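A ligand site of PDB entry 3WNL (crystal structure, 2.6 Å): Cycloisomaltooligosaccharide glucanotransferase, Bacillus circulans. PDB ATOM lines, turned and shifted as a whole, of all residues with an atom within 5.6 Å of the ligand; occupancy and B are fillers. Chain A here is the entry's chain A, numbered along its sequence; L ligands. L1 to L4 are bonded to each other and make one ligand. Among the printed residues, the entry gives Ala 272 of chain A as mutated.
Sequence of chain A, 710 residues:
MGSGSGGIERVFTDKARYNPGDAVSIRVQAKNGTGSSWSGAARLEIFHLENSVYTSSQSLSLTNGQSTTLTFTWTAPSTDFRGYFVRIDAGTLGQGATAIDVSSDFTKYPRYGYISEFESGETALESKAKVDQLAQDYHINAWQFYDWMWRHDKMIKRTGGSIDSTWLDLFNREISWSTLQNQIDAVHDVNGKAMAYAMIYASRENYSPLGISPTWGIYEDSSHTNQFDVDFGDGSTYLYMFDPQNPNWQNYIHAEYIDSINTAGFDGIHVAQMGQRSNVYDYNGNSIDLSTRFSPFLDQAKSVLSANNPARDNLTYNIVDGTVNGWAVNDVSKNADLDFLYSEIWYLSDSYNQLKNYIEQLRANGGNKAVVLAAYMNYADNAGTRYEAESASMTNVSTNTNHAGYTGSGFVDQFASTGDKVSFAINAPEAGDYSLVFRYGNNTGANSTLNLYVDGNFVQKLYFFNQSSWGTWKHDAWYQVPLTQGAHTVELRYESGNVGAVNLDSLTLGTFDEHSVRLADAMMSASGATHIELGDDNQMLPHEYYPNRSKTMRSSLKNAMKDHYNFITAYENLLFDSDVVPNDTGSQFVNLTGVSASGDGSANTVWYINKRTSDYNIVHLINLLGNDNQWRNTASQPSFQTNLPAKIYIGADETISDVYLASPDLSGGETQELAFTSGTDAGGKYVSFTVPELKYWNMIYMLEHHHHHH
NE2 of Gln 273 sits at hydrogen-bond distance from O of Asn 318 (2.8 Å).
OH of Tyr 546 sits at hydrogen-bond distance from NE2 of Gln 144 (2.9 Å).
OE1 of Glu 544 sits close to NE2 of His 543.
The side-chain hydroxyl of Tyr 546 sits at hydrogen-bond distance from the side-chain hydroxyl of Tyr 342.
The backbone carbonyl oxygen of Glu 544 is in hydrogen-bond range of the side-chain hydroxyl of Tyr 146, at 3.3 Å.
The backbone NH (N) of Gln 273 sits close to the side-chain sulfur (SD) of Met 199, at 3.8 Å.
The backbone NH (N) of Glu 344 is in hydrogen-bond range of the side-chain amide oxygen (OD1) of Asn 318, at 3.2 Å.
N of Tyr 545 lies within hydrogen-bond range of ND1 of His 543 (3.0 Å).
Merely in contact with the ligand: Met 199 (3.2 Å), Tyr 545 (3.2 Å), Tyr 546 (3.5 Å), Phe 465 (3.5 Å), Met 149 (3.6 Å), Asp 476 (3.6 Å), Ala 272 (3.6 Å), Phe 232 (3.8 Å), Phe 171 (3.8 Å), His 543 (3.9 Å), Tyr 376 (3.95 Å) and Met 274 (3.97 Å).
Hydrophobic or aromatic side chains within 4 Å of the ligand: Tyr 146, Met 149, His 152, Phe 171, Tyr 197, Met 199, Phe 232, Ala 272, Met 274, Phe 465, His 543, Tyr 545 and Tyr 546.
Within 4 Å of the ligand: Tyr 146, Asp 147, Met 149, His 152, Phe 171, Tyr 197, Met 199, Phe 232, Ala 272, Gln 273, Met 274, Asn 318, Glu 344, Tyr 376, Phe 465, Asp 476, His 543, Glu 544, Tyr 545, Tyr 546 and Asn 548.
The nearest printed residue that does not touch the ligand is Leu 239 (4.1 Å).
ND2 of Asn 548 sits at hydrogen-bond distance from O1 of LG4 L4 (3.1 Å).
The side-chain carboxylate of Glu 344 is in hydrogen-bond range of an oxygen (O2) of LIG L1 (3.0 Å).
An oxygen (O3) of LG2 L2 sits at hydrogen-bond distance from the side-chain carboxylate (OD2) of Asp 147.
An oxygen (O1) of LG2 L2 is in hydrogen-bond range of the side-chain hydroxyl (OH) of Tyr 197.
A ring nitrogen (NE2) of His 152 lies within hydrogen-bond range of an oxygen (O1) of LG2 L2 (2.8 Å).
The backbone carbonyl oxygen of Glu 544 sits at hydrogen-bond distance from an oxygen (O3) of LIG L1 (2.7 Å).
O1 of LIG L1 sits at hydrogen-bond distance from ND2 of Asn 318, at 3.0 Å.
The side-chain carboxylate (OE2) of Glu 544 sits at hydrogen-bond distance from an oxygen (O1) of LG3 L3.
An oxygen (O1) of LIG L1 is in hydrogen-bond range of the backbone carbonyl oxygen of Gln 273.
An oxygen (O3) of LG2 L2 sits at hydrogen-bond distance from the side-chain hydroxyl (OH) of Tyr 146 (2.7 Å).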
ATOM      1  N   GLN A 144      -6.008  10.397  14.997  1.00  0.00           N
ATOM      2  CA  GLN A 144      -6.917  11.483  15.342  1.00  0.00           C
ATOM      3  C   GLN A 144      -7.936  11.611  14.231  1.00  0.00           C
ATOM      4  O   GLN A 144      -7.602  11.951  13.100  1.00  0.00           O
ATOM      5  CB  GLN A 144      -6.197  12.800  15.571  1.00  0.00           C
ATOM      6  CG  GLN A 144      -6.999  13.859  16.328  1.00  0.00           C
ATOM      7  CD  GLN A 144      -6.512  15.285  16.054  1.00  0.00           C
ATOM      8  OE1 GLN A 144      -7.284  16.208  15.693  1.00  0.00           O
ATOM      9  NE2 GLN A 144      -5.200  15.467  16.186  1.00  0.00           N
ATOM     10  N   TYR A 146     -10.531  13.630  12.606  1.00  0.00           N
ATOM     11  CA  TYR A 146     -10.742  15.058  12.525  1.00  0.00           C
ATOM     12  C   TYR A 146     -11.966  15.371  11.721  1.00  0.00           C
ATOM     13  O   TYR A 146     -12.098  14.934  10.552  1.00  0.00           O
ATOM     14  CB  TYR A 146      -9.573  15.740  11.826  1.00  0.00           C
ATOM     15  CG  TYR A 146      -9.651  17.262  11.842  1.00  0.00           C
ATOM     16  CD1 TYR A 146     -10.389  17.965  10.892  1.00  0.00           C
ATOM     17  CD2 TYR A 146      -8.983  17.984  12.813  1.00  0.00           C
ATOM     18  CE1 TYR A 146     -10.475  19.349  10.939  1.00  0.00           C
ATOM     19  CE2 TYR A 146      -9.050  19.377  12.849  1.00  0.00           C
ATOM     20  CZ  TYR A 146      -9.788  20.040  11.918  1.00  0.00           C
ATOM     21  OH  TYR A 146      -9.836  21.402  11.962  1.00  0.00           O
ATOM     22  N   ASP A 147     -12.807  16.192  12.322  1.00  0.00           N
ATOM     23  CA  ASP A 147     -14.052  16.657  11.711  1.00  0.00           C
ATOM     24  C   ASP A 147     -14.866  15.519  11.181  1.00  0.00           C
ATOM     25  O   ASP A 147     -15.232  15.474   9.997  1.00  0.00           O
ATOM     26  CB  ASP A 147     -13.775  17.711  10.629  1.00  0.00           C
ATOM     27  CG  ASP A 147     -13.652  19.105  11.207  1.00  0.00           C
ATOM     28  OD1 ASP A 147     -13.371  19.169  12.420  1.00  0.00           O
ATOM     29  OD2 ASP A 147     -13.830  20.122  10.470  1.00  0.00           O
ATOM     30  N   MET A 149     -17.503  14.678  13.256  1.00  0.00           N
ATOM     31  CA  MET A 149     -18.771  14.865  13.943  1.00  0.00           C
ATOM     32  C   MET A 149     -19.753  15.644  13.070  1.00  0.00           C
ATOM     33  O   MET A 149     -19.324  16.339  12.174  1.00  0.00           O
ATOM     34  CB  MET A 149     -18.560  15.572  15.282  1.00  0.00           C
ATOM     35  CG  MET A 149     -17.986  16.966  15.214  1.00  0.00           C
ATOM     36  SD  MET A 149     -16.204  16.911  14.989  1.00  0.00           S
ATOM     37  CE  MET A 149     -15.794  18.632  14.759  1.00  0.00           C
ATOM     38  N   HIS A 152     -20.582  20.150  16.699  1.00  0.00           N
ATOM     39  CA  HIS A 152     -19.698  20.190  17.845  1.00  0.00           C
ATOM     40  C   HIS A 152     -20.416  19.842  19.177  1.00  0.00           C
ATOM     41  O   HIS A 152     -19.766  19.353  20.095  1.00  0.00           O
ATOM     42  CB  HIS A 152     -19.059  21.578  17.920  1.00  0.00           C
ATOM     43  CG  HIS A 152     -17.846  21.732  17.044  1.00  0.00           C
ATOM     44  ND1 HIS A 152     -17.930  21.841  15.680  1.00  0.00           N
ATOM     45  CD2 HIS A 152     -16.527  21.736  17.354  1.00  0.00           C
ATOM     46  CE1 HIS A 152     -16.707  21.911  15.175  1.00  0.00           C
ATOM     47  NE2 HIS A 152     -15.846  21.849  16.173  1.00  0.00           N
ATOM     48  N   LEU A 170     -19.697  21.139   9.277  1.00  0.00           N
ATOM     49  CA  LEU A 170     -19.875  22.568   9.282  1.00  0.00           C
ATOM     50  C   LEU A 170     -19.389  23.237   8.003  1.00  0.00           C
ATOM     51  O   LEU A 170     -19.762  24.376   7.741  1.00  0.00           O
ATOM     52  CB  LEU A 170     -19.171  23.210  10.481  1.00  0.00           C
ATOM     53  CG  LEU A 170     -17.641  23.284  10.374  1.00  0.00           C
ATOM     54  CD1 LEU A 170     -16.993  24.228  11.403  1.00  0.00           C
ATOM     55  CD2 LEU A 170     -17.095  21.867  10.516  1.00  0.00           C
ATOM     56  N   PHE A 171     -18.532  22.567   7.252  1.00  0.00           N
ATOM     57  CA  PHE A 171     -18.122  23.082   5.962  1.00  0.00           C
ATOM     58  C   PHE A 171     -18.846  22.347   4.838  1.00  0.00           C
ATOM     59  O   PHE A 171     -18.374  22.286   3.693  1.00  0.00           O
ATOM     60  CB  PHE A 171     -16.627  22.979   5.774  1.00  0.00           C
ATOM     61  CG  PHE A 171     -15.854  23.890   6.666  1.00  0.00           C
ATOM     62  CD1 PHE A 171     -15.867  25.270   6.449  1.00  0.00           C
ATOM     63  CD2 PHE A 171     -15.072  23.381   7.691  1.00  0.00           C
ATOM     64  CE1 PHE A 171     -15.140  26.130   7.264  1.00  0.00           C
ATOM     65  CE2 PHE A 171     -14.341  24.229   8.513  1.00  0.00           C
ATOM     66  CZ  PHE A 171     -14.369  25.608   8.304  1.00  0.00           C
ATOM     67  N   TYR A 197     -11.853  13.599  17.696  1.00  0.00           N
ATOM     68  CA  TYR A 197     -11.667  15.002  17.933  1.00  0.00           C
ATOM     69  C   TYR A 197     -12.958  15.579  18.482  1.00  0.00           C
ATOM     70  O   TYR A 197     -14.071  15.270  18.027  1.00  0.00           O
ATOM     71  CB  TYR A 197     -11.349  15.678  16.623  1.00  0.00           C
ATOM     72  CG  TYR A 197     -11.358  17.218  16.658  1.00  0.00           C
ATOM     73  CD1 TYR A 197     -12.550  17.952  16.666  1.00  0.00           C
ATOM     74  CD2 TYR A 197     -10.178  17.914  16.669  1.00  0.00           C
ATOM     75  CE1 TYR A 197     -12.532  19.325  16.675  1.00  0.00           C
ATOM     76  CE2 TYR A 197     -10.154  19.275  16.651  1.00  0.00           C
ATOM     77  CZ  TYR A 197     -11.312  19.978  16.659  1.00  0.00           C
ATOM     78  OH  TYR A 197     -11.224  21.348  16.662  1.00  0.00           O
ATOM     79  N   MET A 199     -14.272  19.425  20.755  1.00  0.00           N
ATOM     80  CA  MET A 199     -13.928  20.619  21.503  1.00  0.00           C
ATOM     81  C   MET A 199     -14.222  20.451  23.003  1.00  0.00           C
ATOM     82  O   MET A 199     -15.140  19.760  23.390  1.00  0.00           O
ATOM     83  CB  MET A 199     -14.734  21.807  20.971  1.00  0.00           C
ATOM     84  CG  MET A 199     -14.086  22.537  19.802  1.00  0.00           C
ATOM     85  SD  MET A 199     -12.689  23.602  20.296  1.00  0.00           S
ATOM     86  CE  MET A 199     -12.059  24.164  18.738  1.00  0.00           C
ATOM     87  N   VAL A 230     -16.755  31.892  17.432  1.00  0.00           N
ATOM     88  CA  VAL A 230     -15.851  31.634  16.311  1.00  0.00           C
ATOM     89  C   VAL A 230     -16.726  31.797  15.080  1.00  0.00           C
ATOM     90  O   VAL A 230     -17.769  31.152  14.951  1.00  0.00           O
ATOM     91  CB  VAL A 230     -15.235  30.223  16.375  1.00  0.00           C
ATOM     92  CG1 VAL A 230     -14.319  29.977  15.206  1.00  0.00           C
ATOM     93  CG2 VAL A 230     -14.412  30.074  17.633  1.00  0.00           C
ATOM     94  N   PHE A 232     -17.320  31.716  11.163  1.00  0.00           N
ATOM     95  CA  PHE A 232     -16.782  31.039   9.957  1.00  0.00           C
ATOM     96  C   PHE A 232     -16.969  31.803   8.672  1.00  0.00           C
ATOM     97  O   PHE A 232     -16.495  31.353   7.636  1.00  0.00           O
ATOM     98  CB  PHE A 232     -17.311  29.605   9.851  1.00  0.00           C
ATOM     99  CG  PHE A 232     -16.695  28.740  10.863  1.00  0.00           C
ATOM    100  CD1 PHE A 232     -15.355  28.402  10.753  1.00  0.00           C
ATOM    101  CD2 PHE A 232     -17.384  28.396  12.018  1.00  0.00           C
ATOM    102  CE1 PHE A 232     -14.731  27.659  11.720  1.00  0.00           C
ATOM    103  CE2 PHE A 232     -16.782  27.651  12.981  1.00  0.00           C
ATOM    104  CZ  PHE A 232     -15.465  27.261  12.823  1.00  0.00           C
ATOM    105  N   LEU A 239     -19.253  28.639  16.045  1.00  0.00           N
ATOM    106  CA  LEU A 239     -19.134  28.089  17.359  1.00  0.00           C
ATOM    107  C   LEU A 239     -19.316  29.149  18.506  1.00  0.00           C
ATOM    108  O   LEU A 239     -18.700  30.209  18.496  1.00  0.00           O
ATOM    109  CB  LEU A 239     -17.769  27.402  17.504  1.00  0.00           C
ATOM    110  CG  LEU A 239     -17.383  26.349  16.480  1.00  0.00           C
ATOM    111  CD1 LEU A 239     -15.941  25.960  16.770  1.00  0.00           C
ATOM    112  CD2 LEU A 239     -18.258  25.111  16.505  1.00  0.00           C
ATOM    113  N   ALA A 272      -9.863  19.441  21.933  1.00  0.00           N
ATOM    114  CA  ALA A 272      -9.331  20.629  21.331  1.00  0.00           C
ATOM    115  C   ALA A 272      -9.768  21.885  22.053  1.00  0.00           C
ATOM    116  O   ALA A 272     -10.640  21.850  22.937  1.00  0.00           O
ATOM    117  CB  ALA A 272      -9.861  20.683  19.914  1.00  0.00           C
ATOM    118  N   GLN A 273      -9.207  23.016  21.633  1.00  0.00           N
ATOM    119  CA  GLN A 273      -9.593  24.322  22.138  1.00  0.00           C
ATOM    120  C   GLN A 273      -9.079  25.373  21.202  1.00  0.00           C
ATOM    121  O   GLN A 273      -8.243  25.067  20.338  1.00  0.00           O
ATOM    122  CB  GLN A 273      -9.025  24.568  23.520  1.00  0.00           C
ATOM    123  CG  GLN A 273      -7.521  24.599  23.519  1.00  0.00           C
ATOM    124  CD  GLN A 273      -6.921  25.551  24.533  1.00  0.00           C
ATOM    125  OE1 GLN A 273      -7.536  26.554  24.951  1.00  0.00           O
ATOM    126  NE2 GLN A 273      -5.693  25.229  24.957  1.00  0.00           N
ATOM    127  N   MET A 274      -9.561  26.610  21.378  1.00  0.00           N
ATOM    128  CA  MET A 274      -9.169  27.683  20.449  1.00  0.00           C
ATOM    129  C   MET A 274      -7.919  28.428  20.894  1.00  0.00           C
ATOM    130  O   MET A 274      -7.371  29.170  20.172  1.00  0.00           O
ATOM    131  CB  MET A 274     -10.311  28.649  20.220  1.00  0.00           C
ATOM    132  CG  MET A 274     -11.502  28.037  19.508  1.00  0.00           C
ATOM    133  SD  MET A 274     -11.155  27.517  17.797  1.00  0.00           S
ATOM    134  CE  MET A 274     -10.616  29.022  16.998  1.00  0.00           C
ATOM    135  N   ASN A 318      -5.436  19.665  23.706  1.00  0.00           N
ATOM    136  CA  ASN A 318      -4.571  20.556  22.939  1.00  0.00           C
ATOM    137  C   ASN A 318      -4.137  21.807  23.713  1.00  0.00           C
ATOM    138  O   ASN A 318      -4.906  22.808  23.836  1.00  0.00           O
ATOM    139  CB  ASN A 318      -5.244  20.968  21.644  1.00  0.00           C
ATOM    140  CG  ASN A 318      -4.287  21.658  20.689  1.00  0.00           C
ATOM    141  OD1 ASN A 318      -3.053  21.602  20.872  1.00  0.00           O
ATOM    142  ND2 ASN A 318      -4.844  22.314  19.644  1.00  0.00           N
ATOM    143  N   VAL A 320      -2.780  24.763  23.033  1.00  0.00           N
ATOM    144  CA  VAL A 320      -2.577  25.659  21.898  1.00  0.00           C
ATOM    145  C   VAL A 320      -1.557  26.769  22.126  1.00  0.00           C
ATOM    146  O   VAL A 320      -1.558  27.411  23.141  1.00  0.00           O
ATOM    147  CB  VAL A 320      -3.900  26.361  21.529  1.00  0.00           C
ATOM    148  CG1 VAL A 320      -3.679  27.509  20.558  1.00  0.00           C
ATOM    149  CG2 VAL A 320      -4.830  25.358  20.906  1.00  0.00           C
ATOM    150  N   TYR A 342      -0.219  16.999  24.415  1.00  0.00           N
ATOM    151  CA  TYR A 342      -0.312  17.450  23.030  1.00  0.00           C
ATOM    152  C   TYR A 342      -0.305  19.000  22.950  1.00  0.00           C
ATOM    153  O   TYR A 342      -0.899  19.687  23.775  1.00  0.00           O
ATOM    154  CB  TYR A 342      -1.608  16.881  22.443  1.00  0.00           C
ATOM    155  CG  TYR A 342      -1.877  17.152  20.958  1.00  0.00           C
ATOM    156  CD1 TYR A 342      -2.444  18.357  20.529  1.00  0.00           C
ATOM    157  CD2 TYR A 342      -1.641  16.168  20.002  1.00  0.00           C
ATOM    158  CE1 TYR A 342      -2.710  18.605  19.180  1.00  0.00           C
ATOM    159  CE2 TYR A 342      -1.932  16.381  18.653  1.00  0.00           C
ATOM    160  CZ  TYR A 342      -2.457  17.594  18.242  1.00  0.00           C
ATOM    161  OH  TYR A 342      -2.792  17.780  16.919  1.00  0.00           O
ATOM    162  N   GLU A 344      -0.120  22.467  20.021  1.00  0.00           N
ATOM    163  CA  GLU A 344      -0.009  23.054  18.685  1.00  0.00           C
ATOM    164  C   GLU A 344       0.887  24.281  18.794  1.00  0.00           C
ATOM    165  O   GLU A 344       0.574  25.255  19.510  1.00  0.00           O
ATOM    166  CB  GLU A 344      -1.409  23.357  18.186  1.00  0.00           C
ATOM    167  CG  GLU A 344      -1.546  23.903  16.801  1.00  0.00           C
ATOM    168  CD  GLU A 344      -2.995  24.221  16.465  1.00  0.00           C
ATOM    169  OE1 GLU A 344      -3.672  24.970  17.241  1.00  0.00           O
ATOM    170  OE2 GLU A 344      -3.461  23.731  15.416  1.00  0.00           O
ATOM    171  N   TYR A 376       2.845  22.649  11.955  1.00  0.00           N
ATOM    172  CA  TYR A 376       2.677  22.410  10.558  1.00  0.00           C
ATOM    173  C   TYR A 376       3.831  22.982   9.796  1.00  0.00           C
ATOM    174  O   TYR A 376       4.073  24.187   9.800  1.00  0.00           O
ATOM    175  CB  TYR A 376       1.334  22.919  10.086  1.00  0.00           C
ATOM    176  CG  TYR A 376       0.252  22.644  11.117  1.00  0.00           C
ATOM    177  CD1 TYR A 376      -0.088  21.339  11.479  1.00  0.00           C
ATOM    178  CD2 TYR A 376      -0.395  23.689  11.735  1.00  0.00           C
ATOM    179  CE1 TYR A 376      -1.077  21.102  12.458  1.00  0.00           C
ATOM    180  CE2 TYR A 376      -1.373  23.448  12.683  1.00  0.00           C
ATOM    181  CZ  TYR A 376      -1.712  22.159  13.060  1.00  0.00           C
ATOM    182  OH  TYR A 376      -2.691  21.996  14.027  1.00  0.00           O
ATOM    183  N   PHE A 465      -9.684  34.318  -2.489  1.00  0.00           N
ATOM    184  CA  PHE A 465     -10.271  35.118  -1.411  1.00  0.00           C
ATOM    185  C   PHE A 465      -9.982  36.592  -1.548  1.00  0.00           C
ATOM    186  O   PHE A 465      -8.893  36.976  -1.940  1.00  0.00           O
ATOM    187  CB  PHE A 465      -9.780  34.620  -0.060  1.00  0.00           C
ATOM    188  CG  PHE A 465     -10.020  33.152   0.131  1.00  0.00           C
ATOM    189  CD1 PHE A 465     -11.302  32.670   0.231  1.00  0.00           C
ATOM    190  CD2 PHE A 465      -8.968  32.266   0.153  1.00  0.00           C
ATOM    191  CE1 PHE A 465     -11.542  31.343   0.388  1.00  0.00           C
ATOM    192  CE2 PHE A 465      -9.195  30.928   0.295  1.00  0.00           C
ATOM    193  CZ  PHE A 465     -10.479  30.450   0.405  1.00  0.00           C
ATOM    194  N   ASP A 476      -3.401  30.451  -1.001  1.00  0.00           N
ATOM    195  CA  ASP A 476      -4.266  29.515  -0.359  1.00  0.00           C
ATOM    196  C   ASP A 476      -5.408  29.099  -1.314  1.00  0.00           C
ATOM    197  O   ASP A 476      -6.462  28.617  -0.878  1.00  0.00           O
ATOM    198  CB  ASP A 476      -4.790  30.146   0.939  1.00  0.00           C
ATOM    199  CG  ASP A 476      -5.546  31.488   0.707  1.00  0.00           C
ATOM    200  OD1 ASP A 476      -5.476  32.113  -0.384  1.00  0.00           O
ATOM    201  OD2 ASP A 476      -6.240  31.927   1.653  1.00  0.00           O
ATOM    202  N   TRP A 478      -5.714  26.260  -4.013  1.00  0.00           N
ATOM    203  CA  TRP A 478      -4.977  25.072  -4.370  1.00  0.00           C
ATOM    204  C   TRP A 478      -6.011  23.967  -4.671  1.00  0.00           C
ATOM    205  O   TRP A 478      -7.157  24.069  -4.301  1.00  0.00           O
ATOM    206  CB  TRP A 478      -4.006  24.688  -3.214  1.00  0.00           C
ATOM    207  CG  TRP A 478      -4.754  24.527  -1.969  1.00  0.00           C
ATOM    208  CD1 TRP A 478      -5.012  25.489  -1.008  1.00  0.00           C
ATOM    209  CD2 TRP A 478      -5.486  23.391  -1.585  1.00  0.00           C
ATOM    210  NE1 TRP A 478      -5.825  24.971  -0.023  1.00  0.00           N
ATOM    211  CE2 TRP A 478      -6.146  23.694  -0.374  1.00  0.00           C
ATOM    212  CE3 TRP A 478      -5.630  22.128  -2.129  1.00  0.00           C
ATOM    213  CZ2 TRP A 478      -6.945  22.763   0.281  1.00  0.00           C
ATOM    214  CZ3 TRP A 478      -6.403  21.204  -1.450  1.00  0.00           C
ATOM    215  CH2 TRP A 478      -7.054  21.527  -0.269  1.00  0.00           C
ATOM    216  N   HIS A 543      -1.544  22.117   7.584  1.00  0.00           N
ATOM    217  CA  HIS A 543      -2.359  23.219   8.079  1.00  0.00           C
ATOM    218  C   HIS A 543      -3.194  22.663   9.224  1.00  0.00           C
ATOM    219  O   HIS A 543      -3.367  21.466   9.310  1.00  0.00           O
ATOM    220  CB  HIS A 543      -3.235  23.691   6.913  1.00  0.00           C
ATOM    221  CG  HIS A 543      -3.989  24.956   7.161  1.00  0.00           C
ATOM    222  ND1 HIS A 543      -5.226  24.975   7.756  1.00  0.00           N
ATOM    223  CD2 HIS A 543      -3.702  26.239   6.822  1.00  0.00           C
ATOM    224  CE1 HIS A 543      -5.680  26.212   7.779  1.00  0.00           C
ATOM    225  NE2 HIS A 543      -4.764  27.004   7.241  1.00  0.00           N
ATOM    226  N   GLU A 544      -3.693  23.531  10.096  1.00  0.00           N
ATOM    227  CA  GLU A 544      -4.585  23.109  11.197  1.00  0.00           C
ATOM    228  C   GLU A 544      -5.952  22.494  10.741  1.00  0.00           C
ATOM    229  O   GLU A 544      -6.589  21.763  11.495  1.00  0.00           O
ATOM    230  CB  GLU A 544      -4.819  24.309  12.128  1.00  0.00           C
ATOM    231  CG  GLU A 544      -5.764  25.403  11.622  1.00  0.00           C
ATOM    232  CD  GLU A 544      -5.062  26.671  11.100  1.00  0.00           C
ATOM    233  OE1 GLU A 544      -3.990  26.598  10.438  1.00  0.00           O
ATOM    234  OE2 GLU A 544      -5.667  27.753  11.289  1.00  0.00           O
ATOM    235  N   TYR A 545      -6.422  22.860   9.550  1.00  0.00           N
ATOM    236  CA  TYR A 545      -7.573  22.217   8.907  1.00  0.00           C
ATOM    237  C   TYR A 545      -6.996  21.018   8.122  1.00  0.00           C
ATOM    238  O   TYR A 545      -6.498  21.148   6.982  1.00  0.00           O
ATOM    239  CB  TYR A 545      -8.363  23.208   7.987  1.00  0.00           C
ATOM    240  CG  TYR A 545      -9.647  22.628   7.420  1.00  0.00           C
ATOM    241  CD1 TYR A 545     -10.724  22.322   8.241  1.00  0.00           C
ATOM    242  CD2 TYR A 545      -9.754  22.285   6.053  1.00  0.00           C
ATOM    243  CE1 TYR A 545     -11.884  21.708   7.730  1.00  0.00           C
ATOM    244  CE2 TYR A 545     -10.905  21.687   5.536  1.00  0.00           C
ATOM    245  CZ  TYR A 545     -11.961  21.404   6.385  1.00  0.00           C
ATOM    246  OH  TYR A 545     -13.091  20.809   5.872  1.00  0.00           O
ATOM    247  N   TYR A 546      -7.044  19.867   8.782  1.00  0.00           N
ATOM    248  CA  TYR A 546      -6.411  18.644   8.339  1.00  0.00           C
ATOM    249  C   TYR A 546      -6.868  18.170   6.922  1.00  0.00           C
ATOM    250  O   TYR A 546      -6.116  17.451   6.239  1.00  0.00           O
ATOM    251  CB  TYR A 546      -6.686  17.510   9.369  1.00  0.00           C
ATOM    252  CG  TYR A 546      -6.010  17.555  10.749  1.00  0.00           C
ATOM    253  CD1 TYR A 546      -5.514  18.729  11.303  1.00  0.00           C
ATOM    254  CD2 TYR A 546      -5.928  16.406  11.540  1.00  0.00           C
ATOM    255  CE1 TYR A 546      -4.891  18.729  12.545  1.00  0.00           C
ATOM    256  CE2 TYR A 546      -5.348  16.416  12.812  1.00  0.00           C
ATOM    257  CZ  TYR A 546      -4.814  17.577  13.290  1.00  0.00           C
ATOM    258  OH  TYR A 546      -4.223  17.603  14.524  1.00  0.00           O
ATOM    259  N   ASN A 548      -6.871  19.853   4.405  1.00  0.00           N
ATOM    260  CA  ASN A 548      -6.072  20.690   3.524  1.00  0.00           C
ATOM    261  C   ASN A 548      -4.954  19.903   2.867  1.00  0.00           C
ATOM    262  O   ASN A 548      -4.213  19.261   3.562  1.00  0.00           O
ATOM    263  CB  ASN A 548      -5.447  21.790   4.393  1.00  0.00           C
ATOM    264  CG  ASN A 548      -4.527  22.714   3.633  1.00  0.00           C
ATOM    265  OD1 ASN A 548      -3.394  22.352   3.250  1.00  0.00           O
ATOM    266  ND2 ASN A 548      -4.945  23.953   3.517  1.00  0.00           N
HETATM  267  C1  LIG L   1      -6.949  22.255  16.323  1.00  0.00           C
HETATM  268  C2  LIG L   1      -6.984  22.506  14.833  1.00  0.00           C
HETATM  269  C3  LIG L   1      -8.325  23.069  14.380  1.00  0.00           C
HETATM  270  C4  LIG L   1      -8.694  24.222  15.314  1.00  0.00           C
HETATM  271  C5  LIG L   1      -9.981  25.006  14.959  1.00  0.00           C
HETATM  272  C6  LIG L   1      -7.479  23.429  17.109  1.00  0.00           C
HETATM  273  O1  LIG L   1      -7.526  23.066  18.499  1.00  0.00           O
HETATM  274  O2  LIG L   1      -5.602  22.042  16.699  1.00  0.00           O
HETATM  275  O3  LIG L   1      -6.662  21.291  14.122  1.00  0.00           O
HETATM  276  O4  LIG L   1      -8.175  23.572  13.037  1.00  0.00           O
HETATM  277  O5  LIG L   1      -8.774  23.678  16.614  1.00  0.00           O
HETATM  278  O6  LIG L   1     -11.073  24.099  14.957  1.00  0.00           O
HETATM  279  C1  LG2 L   2     -12.334  24.673  14.653  1.00  0.00           C
HETATM  280  C2  LG2 L   2     -13.334  23.495  14.757  1.00  0.00           C
HETATM  281  C3  LG2 L   2     -12.973  22.455  13.698  1.00  0.00           C
HETATM  282  C4  LG2 L   2     -12.799  23.097  12.316  1.00  0.00           C
HETATM  283  C5  LG2 L   2     -11.833  24.325  12.395  1.00  0.00           C
HETATM  284  C6  LG2 L   2     -11.761  25.144  11.119  1.00  0.00           C
HETATM  285  O1  LG2 L   2     -13.273  22.882  16.043  1.00  0.00           O
HETATM  286  O2  LG2 L   2     -14.003  21.527  13.663  1.00  0.00           O
HETATM  287  O3  LG2 L   2     -12.359  22.110  11.419  1.00  0.00           O
HETATM  288  O4  LG2 L   2     -12.348  25.227  13.338  1.00  0.00           O
HETATM  289  O5  LG2 L   2     -10.936  26.312  11.286  1.00  0.00           O
HETATM  290  C1  LG3 L   3      -9.633  26.186  10.656  1.00  0.00           C
HETATM  291  C2  LG3 L   3      -8.864  27.481  10.829  1.00  0.00           C
HETATM  292  C3  LG3 L   3      -9.549  28.596  10.076  1.00  0.00           C
HETATM  293  C4  LG3 L   3      -9.758  28.213   8.615  1.00  0.00           C
HETATM  294  C5  LG3 L   3     -10.378  26.807   8.451  1.00  0.00           C
HETATM  295  C6  LG3 L   3     -10.566  26.368   6.999  1.00  0.00           C
HETATM  296  O1  LG3 L   3      -8.720  27.847  12.181  1.00  0.00           O
HETATM  297  O2  LG3 L   3      -8.579  29.601  10.105  1.00  0.00           O
HETATM  298  O3  LG3 L   3     -10.650  29.119   8.030  1.00  0.00           O
HETATM  299  O4  LG3 L   3      -9.632  25.882   9.261  1.00  0.00           O
HETATM  300  O5  LG3 L   3      -9.358  26.543   6.237  1.00  0.00           O
HETATM  301  C1  LG4 L   4      -9.603  26.408   4.817  1.00  0.00           C
HETATM  302  C2  LG4 L   4      -8.251  26.300   4.111  1.00  0.00           C
HETATM  303  C3  LG4 L   4      -7.451  27.610   4.306  1.00  0.00           C
HETATM  304  C4  LG4 L   4      -8.299  28.868   3.969  1.00  0.00           C
HETATM  305  C5  LG4 L   4      -9.787  28.819   4.470  1.00  0.00           C
HETATM  306  C6  LG4 L   4     -10.744  29.896   3.867  1.00  0.00           C
HETATM  307  O1  LG4 L   4      -7.573  25.136   4.557  1.00  0.00           O
HETATM  308  O2  LG4 L   4      -6.248  27.637   3.557  1.00  0.00           O
HETATM  309  O3  LG4 L   4      -7.558  30.010   4.401  1.00  0.00           O
HETATM  310  O4  LG4 L   4     -10.328  27.510   4.232  1.00  0.00           O
HETATM  311  O5  LG4 L   4     -11.937  30.238   4.598  1.00  0.00           O
